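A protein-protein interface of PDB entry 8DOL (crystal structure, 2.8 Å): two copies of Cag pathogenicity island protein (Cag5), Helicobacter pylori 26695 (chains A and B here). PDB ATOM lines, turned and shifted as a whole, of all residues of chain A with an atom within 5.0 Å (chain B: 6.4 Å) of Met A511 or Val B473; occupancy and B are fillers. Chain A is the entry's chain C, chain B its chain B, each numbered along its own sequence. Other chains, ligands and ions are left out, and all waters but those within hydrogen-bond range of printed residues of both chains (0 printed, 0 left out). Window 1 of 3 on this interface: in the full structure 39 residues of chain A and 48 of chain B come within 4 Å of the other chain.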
ATOM      1  N   GLY A 457      -4.823  19.687   0.864  1.00  0.00           N
ATOM      2  CA  GLY A 457      -5.052  18.296   0.503  1.00  0.00           C
ATOM      3  C   GLY A 457      -6.148  17.672   1.348  1.00  0.00           C
ATOM      4  O   GLY A 457      -6.211  17.892   2.561  1.00  0.00           O
ATOM      5  N   ILE A 458      -7.015  16.899   0.693  1.00  0.00           N
ATOM      6  CA  ILE A 458      -8.023  16.100   1.376  1.00  0.00           C
ATOM      7  C   ILE A 458      -8.125  14.754   0.677  1.00  0.00           C
ATOM      8  O   ILE A 458      -7.954  14.649  -0.542  1.00  0.00           O
ATOM      9  CB  ILE A 458      -9.405  16.788   1.417  1.00  0.00           C
ATOM     10  CG1 ILE A 458      -9.891  17.091  -0.001  1.00  0.00           C
ATOM     11  CG2 ILE A 458      -9.367  18.041   2.286  1.00  0.00           C
ATOM     12  CD1 ILE A 458     -11.390  17.009  -0.146  1.00  0.00           C
ATOM     13  N   ASN A 459      -8.409  13.714   1.463  1.00  0.00           N
ATOM     14  CA  ASN A 459      -8.489  12.345   0.957  1.00  0.00           C
ATOM     15  C   ASN A 459      -9.925  12.071   0.516  1.00  0.00           C
ATOM     16  O   ASN A 459     -10.710  11.408   1.200  1.00  0.00           O
ATOM     17  CB  ASN A 459      -8.017  11.360   2.019  1.00  0.00           C
ATOM     18  CG  ASN A 459      -7.796   9.969   1.468  1.00  0.00           C
ATOM     19  OD1 ASN A 459      -7.717   9.772   0.255  1.00  0.00           O
ATOM     20  ND2 ASN A 459      -7.697   8.990   2.361  1.00  0.00           N
ATOM     21  N   ASN A 460     -10.268  12.602  -0.655  1.00  0.00           N
ATOM     22  CA  ASN A 460     -11.601  12.468  -1.230  1.00  0.00           C
ATOM     23  C   ASN A 460     -11.462  12.018  -2.676  1.00  0.00           C
ATOM     24  O   ASN A 460     -10.836  12.711  -3.485  1.00  0.00           O
ATOM     25  CB  ASN A 460     -12.375  13.788  -1.148  1.00  0.00           C
ATOM     26  CG  ASN A 460     -13.864  13.617  -1.395  1.00  0.00           C
ATOM     27  OD1 ASN A 460     -14.304  12.630  -1.985  1.00  0.00           O
ATOM     28  ND2 ASN A 460     -14.651  14.587  -0.944  1.00  0.00           N
ATOM     29  N   ASP A 461     -12.060  10.870  -2.996  1.00  0.00           N
ATOM     30  CA  ASP A 461     -11.934  10.287  -4.330  1.00  0.00           C
ATOM     31  C   ASP A 461     -12.306  11.284  -5.425  1.00  0.00           C
ATOM     32  O   ASP A 461     -11.671  11.319  -6.487  1.00  0.00           O
ATOM     33  CB  ASP A 461     -12.801   9.031  -4.407  1.00  0.00           C
ATOM     34  CG  ASP A 461     -13.210   8.686  -5.812  1.00  0.00           C
ATOM     35  OD1 ASP A 461     -12.351   8.201  -6.575  1.00  0.00           O
ATOM     36  OD2 ASP A 461     -14.395   8.888  -6.147  1.00  0.00           O
ATOM     37  N   TYR A 463     -11.593  14.191  -5.774  1.00  0.00           N
ATOM     38  CA  TYR A 463     -10.503  15.107  -6.068  1.00  0.00           C
ATOM     39  C   TYR A 463      -9.308  14.419  -6.715  1.00  0.00           C
ATOM     40  O   TYR A 463      -8.282  15.076  -6.933  1.00  0.00           O
ATOM     41  CB  TYR A 463     -10.042  15.808  -4.788  1.00  0.00           C
ATOM     42  CG  TYR A 463     -10.869  17.003  -4.369  1.00  0.00           C
ATOM     43  CD1 TYR A 463     -12.081  16.840  -3.707  1.00  0.00           C
ATOM     44  CD2 TYR A 463     -10.423  18.297  -4.609  1.00  0.00           C
ATOM     45  CE1 TYR A 463     -12.828  17.933  -3.307  1.00  0.00           C
ATOM     46  CE2 TYR A 463     -11.163  19.393  -4.214  1.00  0.00           C
ATOM     47  CZ  TYR A 463     -12.364  19.206  -3.565  1.00  0.00           C
ATOM     48  OH  TYR A 463     -13.100  20.301  -3.173  1.00  0.00           O
ATOM     49  N   TYR A 464      -9.413  13.122  -7.024  1.00  0.00           N
ATOM     50  CA  TYR A 464      -8.259  12.386  -7.531  1.00  0.00           C
ATOM     51  C   TYR A 464      -7.648  13.078  -8.745  1.00  0.00           C
ATOM     52  O   TYR A 464      -6.469  13.449  -8.736  1.00  0.00           O
ATOM     53  CB  TYR A 464      -8.646  10.950  -7.883  1.00  0.00           C
ATOM     54  CG  TYR A 464      -7.506  10.186  -8.523  1.00  0.00           C
ATOM     55  CD1 TYR A 464      -6.391   9.814  -7.781  1.00  0.00           C
ATOM     56  CD2 TYR A 464      -7.533   9.862  -9.872  1.00  0.00           C
ATOM     57  CE1 TYR A 464      -5.342   9.122  -8.361  1.00  0.00           C
ATOM     58  CE2 TYR A 464      -6.487   9.173 -10.463  1.00  0.00           C
ATOM     59  CZ  TYR A 464      -5.396   8.806  -9.703  1.00  0.00           C
ATOM     60  OH  TYR A 464      -4.355   8.122 -10.290  1.00  0.00           O
ATOM     61  N   PHE A 467      -5.547  16.099  -7.915  1.00  0.00           N
ATOM     62  CA  PHE A 467      -4.255  15.951  -7.256  1.00  0.00           C
ATOM     63  C   PHE A 467      -3.263  15.188  -8.123  1.00  0.00           C
ATOM     64  O   PHE A 467      -2.070  15.512  -8.128  1.00  0.00           O
ATOM     65  CB  PHE A 467      -4.439  15.271  -5.902  1.00  0.00           C
ATOM     66  CG  PHE A 467      -5.005  16.183  -4.850  1.00  0.00           C
ATOM     67  CD1 PHE A 467      -4.301  17.305  -4.441  1.00  0.00           C
ATOM     68  CD2 PHE A 467      -6.247  15.936  -4.291  1.00  0.00           C
ATOM     69  CE1 PHE A 467      -4.819  18.154  -3.485  1.00  0.00           C
ATOM     70  CE2 PHE A 467      -6.770  16.783  -3.333  1.00  0.00           C
ATOM     71  CZ  PHE A 467      -6.055  17.892  -2.929  1.00  0.00           C
ATOM     72  N   PRO A 507       0.023  11.217  -5.881  1.00  0.00           N
ATOM     73  CA  PRO A 507      -1.330  11.756  -5.644  1.00  0.00           C
ATOM     74  C   PRO A 507      -1.873  11.454  -4.257  1.00  0.00           C
ATOM     75  O   PRO A 507      -2.404  12.355  -3.594  1.00  0.00           O
ATOM     76  CB  PRO A 507      -2.162  11.086  -6.745  1.00  0.00           C
ATOM     77  CG  PRO A 507      -1.189  10.824  -7.837  1.00  0.00           C
ATOM     78  CD  PRO A 507       0.111  10.491  -7.160  1.00  0.00           C
ATOM     79  N   ASP A 508      -1.755  10.208  -3.794  1.00  0.00           N
ATOM     80  CA  ASP A 508      -2.263   9.866  -2.470  1.00  0.00           C
ATOM     81  C   ASP A 508      -1.453  10.517  -1.356  1.00  0.00           C
ATOM     82  O   ASP A 508      -1.959  10.655  -0.237  1.00  0.00           O
ATOM     83  CB  ASP A 508      -2.291   8.348  -2.291  1.00  0.00           C
ATOM     84  CG  ASP A 508      -0.911   7.725  -2.344  1.00  0.00           C
ATOM     85  OD1 ASP A 508      -0.440   7.424  -3.462  1.00  0.00           O
ATOM     86  OD2 ASP A 508      -0.301   7.533  -1.267  1.00  0.00           O
ATOM     87  N   GLU A 509      -0.209  10.917  -1.632  1.00  0.00           N
ATOM     88  CA  GLU A 509       0.556  11.665  -0.641  1.00  0.00           C
ATOM     89  C   GLU A 509       0.060  13.102  -0.547  1.00  0.00           C
ATOM     90  O   GLU A 509      -0.037  13.662   0.552  1.00  0.00           O
ATOM     91  CB  GLU A 509       2.044  11.622  -0.984  1.00  0.00           C
ATOM     92  CG  GLU A 509       2.781  10.418  -0.413  1.00  0.00           C
ATOM     93  CD  GLU A 509       4.048  10.095  -1.185  1.00  0.00           C
ATOM     94  OE1 GLU A 509       4.258  10.702  -2.257  1.00  0.00           O
ATOM     95  OE2 GLU A 509       4.837   9.246  -0.716  1.00  0.00           O
ATOM     96  N   LEU A 510      -0.261  13.712  -1.690  1.00  0.00           N
ATOM     97  CA  LEU A 510      -0.882  15.031  -1.675  1.00  0.00           C
ATOM     98  C   LEU A 510      -2.237  14.986  -0.984  1.00  0.00           C
ATOM     99  O   LEU A 510      -2.595  15.902  -0.233  1.00  0.00           O
ATOM    100  CB  LEU A 510      -1.035  15.552  -3.102  1.00  0.00           C
ATOM    101  CG  LEU A 510       0.220  16.151  -3.730  1.00  0.00           C
ATOM    102  CD1 LEU A 510       0.071  16.226  -5.242  1.00  0.00           C
ATOM    103  CD2 LEU A 510       0.480  17.517  -3.141  1.00  0.00           C
ATOM    104  N   MET A 511      -2.998  13.916  -1.221  1.00  0.00           N
ATOM    105  CA  MET A 511      -4.326  13.793  -0.635  1.00  0.00           C
ATOM    106  C   MET A 511      -4.284  13.698   0.884  1.00  0.00           C
ATOM    107  O   MET A 511      -5.274  14.041   1.539  1.00  0.00           O
ATOM    108  CB  MET A 511      -5.027  12.567  -1.214  1.00  0.00           C
ATOM    109  CG  MET A 511      -5.954  12.876  -2.367  1.00  0.00           C
ATOM    110  SD  MET A 511      -6.253  11.406  -3.356  1.00  0.00           S
ATOM    111  CE  MET A 511      -8.009  11.550  -3.639  1.00  0.00           C
ATOM    112  N   THR A 512      -3.165  13.256   1.462  1.00  0.00           N
ATOM    113  CA  THR A 512      -3.067  13.028   2.899  1.00  0.00           C
ATOM    114  C   THR A 512      -2.017  13.927   3.552  1.00  0.00           C
ATOM    115  O   THR A 512      -1.427  13.563   4.570  1.00  0.00           O
ATOM    116  CB  THR A 512      -2.782  11.551   3.191  1.00  0.00           C
ATOM    117  OG1 THR A 512      -1.527  11.166   2.616  1.00  0.00           O
ATOM    118  CG2 THR A 512      -3.878  10.669   2.603  1.00  0.00           C
ATOM    119  N   MET A 513      -1.786  15.118   2.983  1.00  0.00           N
ATOM    120  CA  MET A 513      -0.826  16.057   3.562  1.00  0.00           C
ATOM    121  C   MET A 513      -1.206  16.474   4.976  1.00  0.00           C
ATOM    122  O   MET A 513      -0.327  16.784   5.787  1.00  0.00           O
ATOM    123  CB  MET A 513      -0.713  17.312   2.697  1.00  0.00           C
ATOM    124  CG  MET A 513      -0.003  17.133   1.384  1.00  0.00           C
ATOM    125  SD  MET A 513       0.327  18.741   0.650  1.00  0.00           S
ATOM    126  CE  MET A 513      -1.221  19.037  -0.188  1.00  0.00           C
ATOM    127  N   GLU B 468     -11.446   0.855 -10.255  1.00  0.00           N
ATOM    128  CA  GLU B 468     -10.076   1.117 -10.685  1.00  0.00           C
ATOM    129  C   GLU B 468      -9.605   2.458 -10.148  1.00  0.00           C
ATOM    130  O   GLU B 468      -8.552   2.549  -9.500  1.00  0.00           O
ATOM    131  CB  GLU B 468      -9.977   1.080 -12.210  1.00  0.00           C
ATOM    132  CG  GLU B 468      -8.560   1.265 -12.745  1.00  0.00           C
ATOM    133  CD  GLU B 468      -8.530   1.471 -14.251  1.00  0.00           C
ATOM    134  OE1 GLU B 468      -8.972   2.543 -14.716  1.00  0.00           O
ATOM    135  OE2 GLU B 468      -8.073   0.557 -14.969  1.00  0.00           O
ATOM    136  N   LYS B 469     -10.408   3.504 -10.362  1.00  0.00           N
ATOM    137  CA  LYS B 469     -10.073   4.811  -9.811  1.00  0.00           C
ATOM    138  C   LYS B 469      -9.876   4.715  -8.306  1.00  0.00           C
ATOM    139  O   LYS B 469      -8.877   5.206  -7.766  1.00  0.00           O
ATOM    140  CB  LYS B 469     -11.165   5.825 -10.152  1.00  0.00           C
ATOM    141  CG  LYS B 469     -10.658   7.246 -10.317  1.00  0.00           C
ATOM    142  CD  LYS B 469     -11.810   8.227 -10.390  1.00  0.00           C
ATOM    143  CE  LYS B 469     -11.635   9.354  -9.394  1.00  0.00           C
ATOM    144  NZ  LYS B 469     -12.848  10.213  -9.311  1.00  0.00           N
ATOM    145  N   LEU B 470     -10.798   4.030  -7.622  1.00  0.00           N
ATOM    146  CA  LEU B 470     -10.679   3.886  -6.177  1.00  0.00           C
ATOM    147  C   LEU B 470      -9.348   3.253  -5.809  1.00  0.00           C
ATOM    148  O   LEU B 470      -8.668   3.714  -4.882  1.00  0.00           O
ATOM    149  CB  LEU B 470     -11.845   3.061  -5.636  1.00  0.00           C
ATOM    150  CG  LEU B 470     -12.013   3.008  -4.117  1.00  0.00           C
ATOM    151  CD1 LEU B 470     -11.901   4.390  -3.503  1.00  0.00           C
ATOM    152  CD2 LEU B 470     -13.348   2.371  -3.774  1.00  0.00           C
ATOM    153  N   SER B 471      -8.935   2.227  -6.561  1.00  0.00           N
ATOM    154  CA  SER B 471      -7.628   1.623  -6.337  1.00  0.00           C
ATOM    155  C   SER B 471      -6.538   2.684  -6.394  1.00  0.00           C
ATOM    156  O   SER B 471      -5.757   2.850  -5.447  1.00  0.00           O
ATOM    157  CB  SER B 471      -7.381   0.523  -7.373  1.00  0.00           C
ATOM    158  OG  SER B 471      -6.326  -0.336  -6.980  1.00  0.00           O
ATOM    159  N   LYS B 472      -6.514   3.460  -7.484  1.00  0.00           N
ATOM    160  CA  LYS B 472      -5.505   4.500  -7.627  1.00  0.00           C
ATOM    161  C   LYS B 472      -5.586   5.516  -6.498  1.00  0.00           C
ATOM    162  O   LYS B 472      -4.559   6.076  -6.095  1.00  0.00           O
ATOM    163  CB  LYS B 472      -5.652   5.195  -8.981  1.00  0.00           C
ATOM    164  CG  LYS B 472      -5.089   4.410 -10.156  1.00  0.00           C
ATOM    165  CD  LYS B 472      -5.991   4.532 -11.372  1.00  0.00           C
ATOM    166  CE  LYS B 472      -5.199   4.831 -12.632  1.00  0.00           C
ATOM    167  NZ  LYS B 472      -6.055   5.498 -13.660  1.00  0.00           N
ATOM    168  N   VAL B 473      -6.787   5.753  -5.960  1.00  0.00           N
ATOM    169  CA  VAL B 473      -6.910   6.741  -4.894  1.00  0.00           C
ATOM    170  C   VAL B 473      -6.262   6.228  -3.617  1.00  0.00           C
ATOM    171  O   VAL B 473      -5.685   7.009  -2.848  1.00  0.00           O
ATOM    172  CB  VAL B 473      -8.387   7.117  -4.674  1.00  0.00           C
ATOM    173  CG1 VAL B 473      -8.565   7.877  -3.370  1.00  0.00           C
ATOM    174  CG2 VAL B 473      -8.897   7.942  -5.841  1.00  0.00           C
ATOM    175  N   LEU B 474      -6.310   4.915  -3.377  1.00  0.00           N
ATOM    176  CA  LEU B 474      -5.725   4.399  -2.146  1.00  0.00           C
ATOM    177  C   LEU B 474      -4.204   4.449  -2.176  1.00  0.00           C
ATOM    178  O   LEU B 474      -3.576   4.428  -1.114  1.00  0.00           O
ATOM    179  CB  LEU B 474      -6.211   2.973  -1.881  1.00  0.00           C
ATOM    180  CG  LEU B 474      -7.720   2.819  -1.658  1.00  0.00           C
ATOM    181  CD1 LEU B 474      -8.063   1.438  -1.125  1.00  0.00           C
ATOM    182  CD2 LEU B 474      -8.230   3.888  -0.715  1.00  0.00           C
ATOM    183  N   GLY B 475      -3.603   4.538  -3.362  1.00  0.00           N
ATOM    184  CA  GLY B 475      -2.162   4.616  -3.477  1.00  0.00           C
ATOM    185  C   GLY B 475      -1.493   3.267  -3.306  1.00  0.00           C
ATOM    186  O   GLY B 475      -2.130   2.231  -3.103  1.00  0.00           O
ATOM    187  N   LEU B 520     -13.247   6.627   3.400  1.00  0.00           N
ATOM    188  CA  LEU B 520     -12.333   7.729   3.124  1.00  0.00           C
ATOM    189  C   LEU B 520     -12.883   8.974   3.803  1.00  0.00           C
ATOM    190  O   LEU B 520     -13.936   9.486   3.405  1.00  0.00           O
ATOM    191  CB  LEU B 520     -12.172   7.964   1.624  1.00  0.00           C
ATOM    192  CG  LEU B 520     -11.528   6.885   0.757  1.00  0.00           C
ATOM    193  CD1 LEU B 520     -11.363   7.404  -0.664  1.00  0.00           C
ATOM    194  CD2 LEU B 520     -10.195   6.443   1.331  1.00  0.00           C
ATOM    195  N   ASN B 522     -11.910  12.991   4.792  1.00  0.00           N
ATOM    196  CA  ASN B 522     -11.075  14.003   4.149  1.00  0.00           C
ATOM    197  C   ASN B 522      -9.740  14.172   4.863  1.00  0.00           C
ATOM    198  O   ASN B 522      -8.708  14.393   4.219  1.00  0.00           O
ATOM    199  CB  ASN B 522     -11.819  15.340   4.094  1.00  0.00           C
ATOM    200  CG  ASN B 522     -12.965  15.333   3.101  1.00  0.00           C
ATOM    201  OD1 ASN B 522     -13.203  14.340   2.413  1.00  0.00           O
ATOM    202  ND2 ASN B 522     -13.685  16.446   3.023  1.00  0.00           N
ATOM    203  N   THR B 523      -9.734  14.054   6.190  1.00  0.00           N
ATOM    204  CA  THR B 523      -8.558  14.343   6.998  1.00  0.00           C
ATOM    205  C   THR B 523      -7.831  13.089   7.470  1.00  0.00           C
ATOM    206  O   THR B 523      -6.945  13.187   8.326  1.00  0.00           O
ATOM    207  CB  THR B 523      -8.953  15.193   8.208  1.00  0.00           C
ATOM    208  OG1 THR B 523      -9.488  14.348   9.233  1.00  0.00           O
ATOM    209  CG2 THR B 523      -9.999  16.223   7.816  1.00  0.00           C
ATOM    210  N   LEU B 524      -8.170  11.921   6.934  1.00  0.00           N
ATOM    211  CA  LEU B 524      -7.616  10.665   7.415  1.00  0.00           C
ATOM    212  C   LEU B 524      -7.108   9.828   6.251  1.00  0.00           C
ATOM    213  O   LEU B 524      -7.501  10.016   5.098  1.00  0.00           O
ATOM    214  CB  LEU B 524      -8.660   9.867   8.206  1.00  0.00           C
ATOM    215  CG  LEU B 524      -9.172  10.484   9.506  1.00  0.00           C
ATOM    216  CD1 LEU B 524      -9.967   9.458  10.277  1.00  0.00           C
ATOM    217  CD2 LEU B 524      -8.025  11.008  10.351  1.00  0.00           C
ATOM    218  N   PRO B 526      -6.866   6.107   4.322  1.00  0.00           N
ATOM    219  CA  PRO B 526      -7.959   5.162   4.052  1.00  0.00           C
ATOM    220  C   PRO B 526      -8.151   4.161   5.182  1.00  0.00           C
ATOM    221  O   PRO B 526      -7.206   3.774   5.873  1.00  0.00           O
ATOM    222  CB  PRO B 526      -7.517   4.464   2.759  1.00  0.00           C
ATOM    223  CG  PRO B 526      -6.072   4.814   2.584  1.00  0.00           C
ATOM    224  CD  PRO B 526      -5.901   6.151   3.213  1.00  0.00           C
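Among the printed residues, merely in contact across the chains: Asp A508 with Gly B475 (3.3 Å), Ile A458 with Asn B522 (3.4 Å), Tyr A464 with Lys B472 (3.5 Å), Asn A459 with Pro B526 (3.5 Å), Asp A461 with Val B473 (3.5 Å), Tyr A464 with Val B473 (3.6 Å), Asn A460 with Asn B522 (3.7 Å), Asp A508 with Val B473 (3.7 Å), Tyr A464 with Lys B469 (3.7 Å), Asn A459 with Leu B520 (3.7 Å) and Met A511 with Val B473 (3.7 Å).
The backbone carbonyl oxygen (O) of Met A511 lies close to the backbone NH (N) of Ile A458 (3.5 Å).
The backbone NH (N) of Asn A459 is in hydrogen-bond range of the backbone carbonyl oxygen (O) of Met A511 (3.2 Å).
The backbone carbonyl oxygen (O) of Asp A508 is in hydrogen-bond range of the side-chain hydroxyl (OG1) of Thr A512, at 2.9 Å.
Of the 15 printed residues of chain A, 7 touch a printed residue of chain B.
Hydrophobic or aromatic side chains of chain A that line the printed part of chain B: Ile A458, Tyr A464 and Met A511.
Of the 13 printed residues of chain B, 8 touch a printed residue of chain A.
Hydrophobic or aromatic side chains of chain B within 4 Å of the printed part of chain A: Val B473, Leu B520 and Pro B526.
Among the printed residues, Asp or Glu carboxylates within 4 Å of a Lys or Arg side-chain nitrogen of the other chain: Asp A461 with Lys B469.
Printed residues of chain B within 4 Å of Asp A461: Lys B469 (3.1 Å) and Val B473 (3.5 Å).
Met A511 touches one residue of chain B.
Leu B470 touches none of the printed residues of chain A.
Of the printed residues of chain A, Lys B472 touches Tyr A464 (3.5 Å).
Val B473 touches just these residues of chain A: Asp A461 (3.5 Å), Tyr A464 (3.6 Å), Asp A508 (3.7 Å) and Met A511 (3.7 Å).
The nearest residue of chain A that does not touch Val B473 is Asn A459 (4.2 Å).
The nearest printed residue of chain B that does not touch Asp A461 is Leu B520 (4.2 Å).
O of Asn B522 sits at hydrogen-bond distance from N of Asn A459 (2.9 Å).
O of Leu B524 is in hydrogen-bond range of ND2 of Asn A459, 2.9 Å away.
NZ of Lys B469 is in salt-bridge range of OD1 of Asp A461, 3.4 Å away.
No position is printed for both chains.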
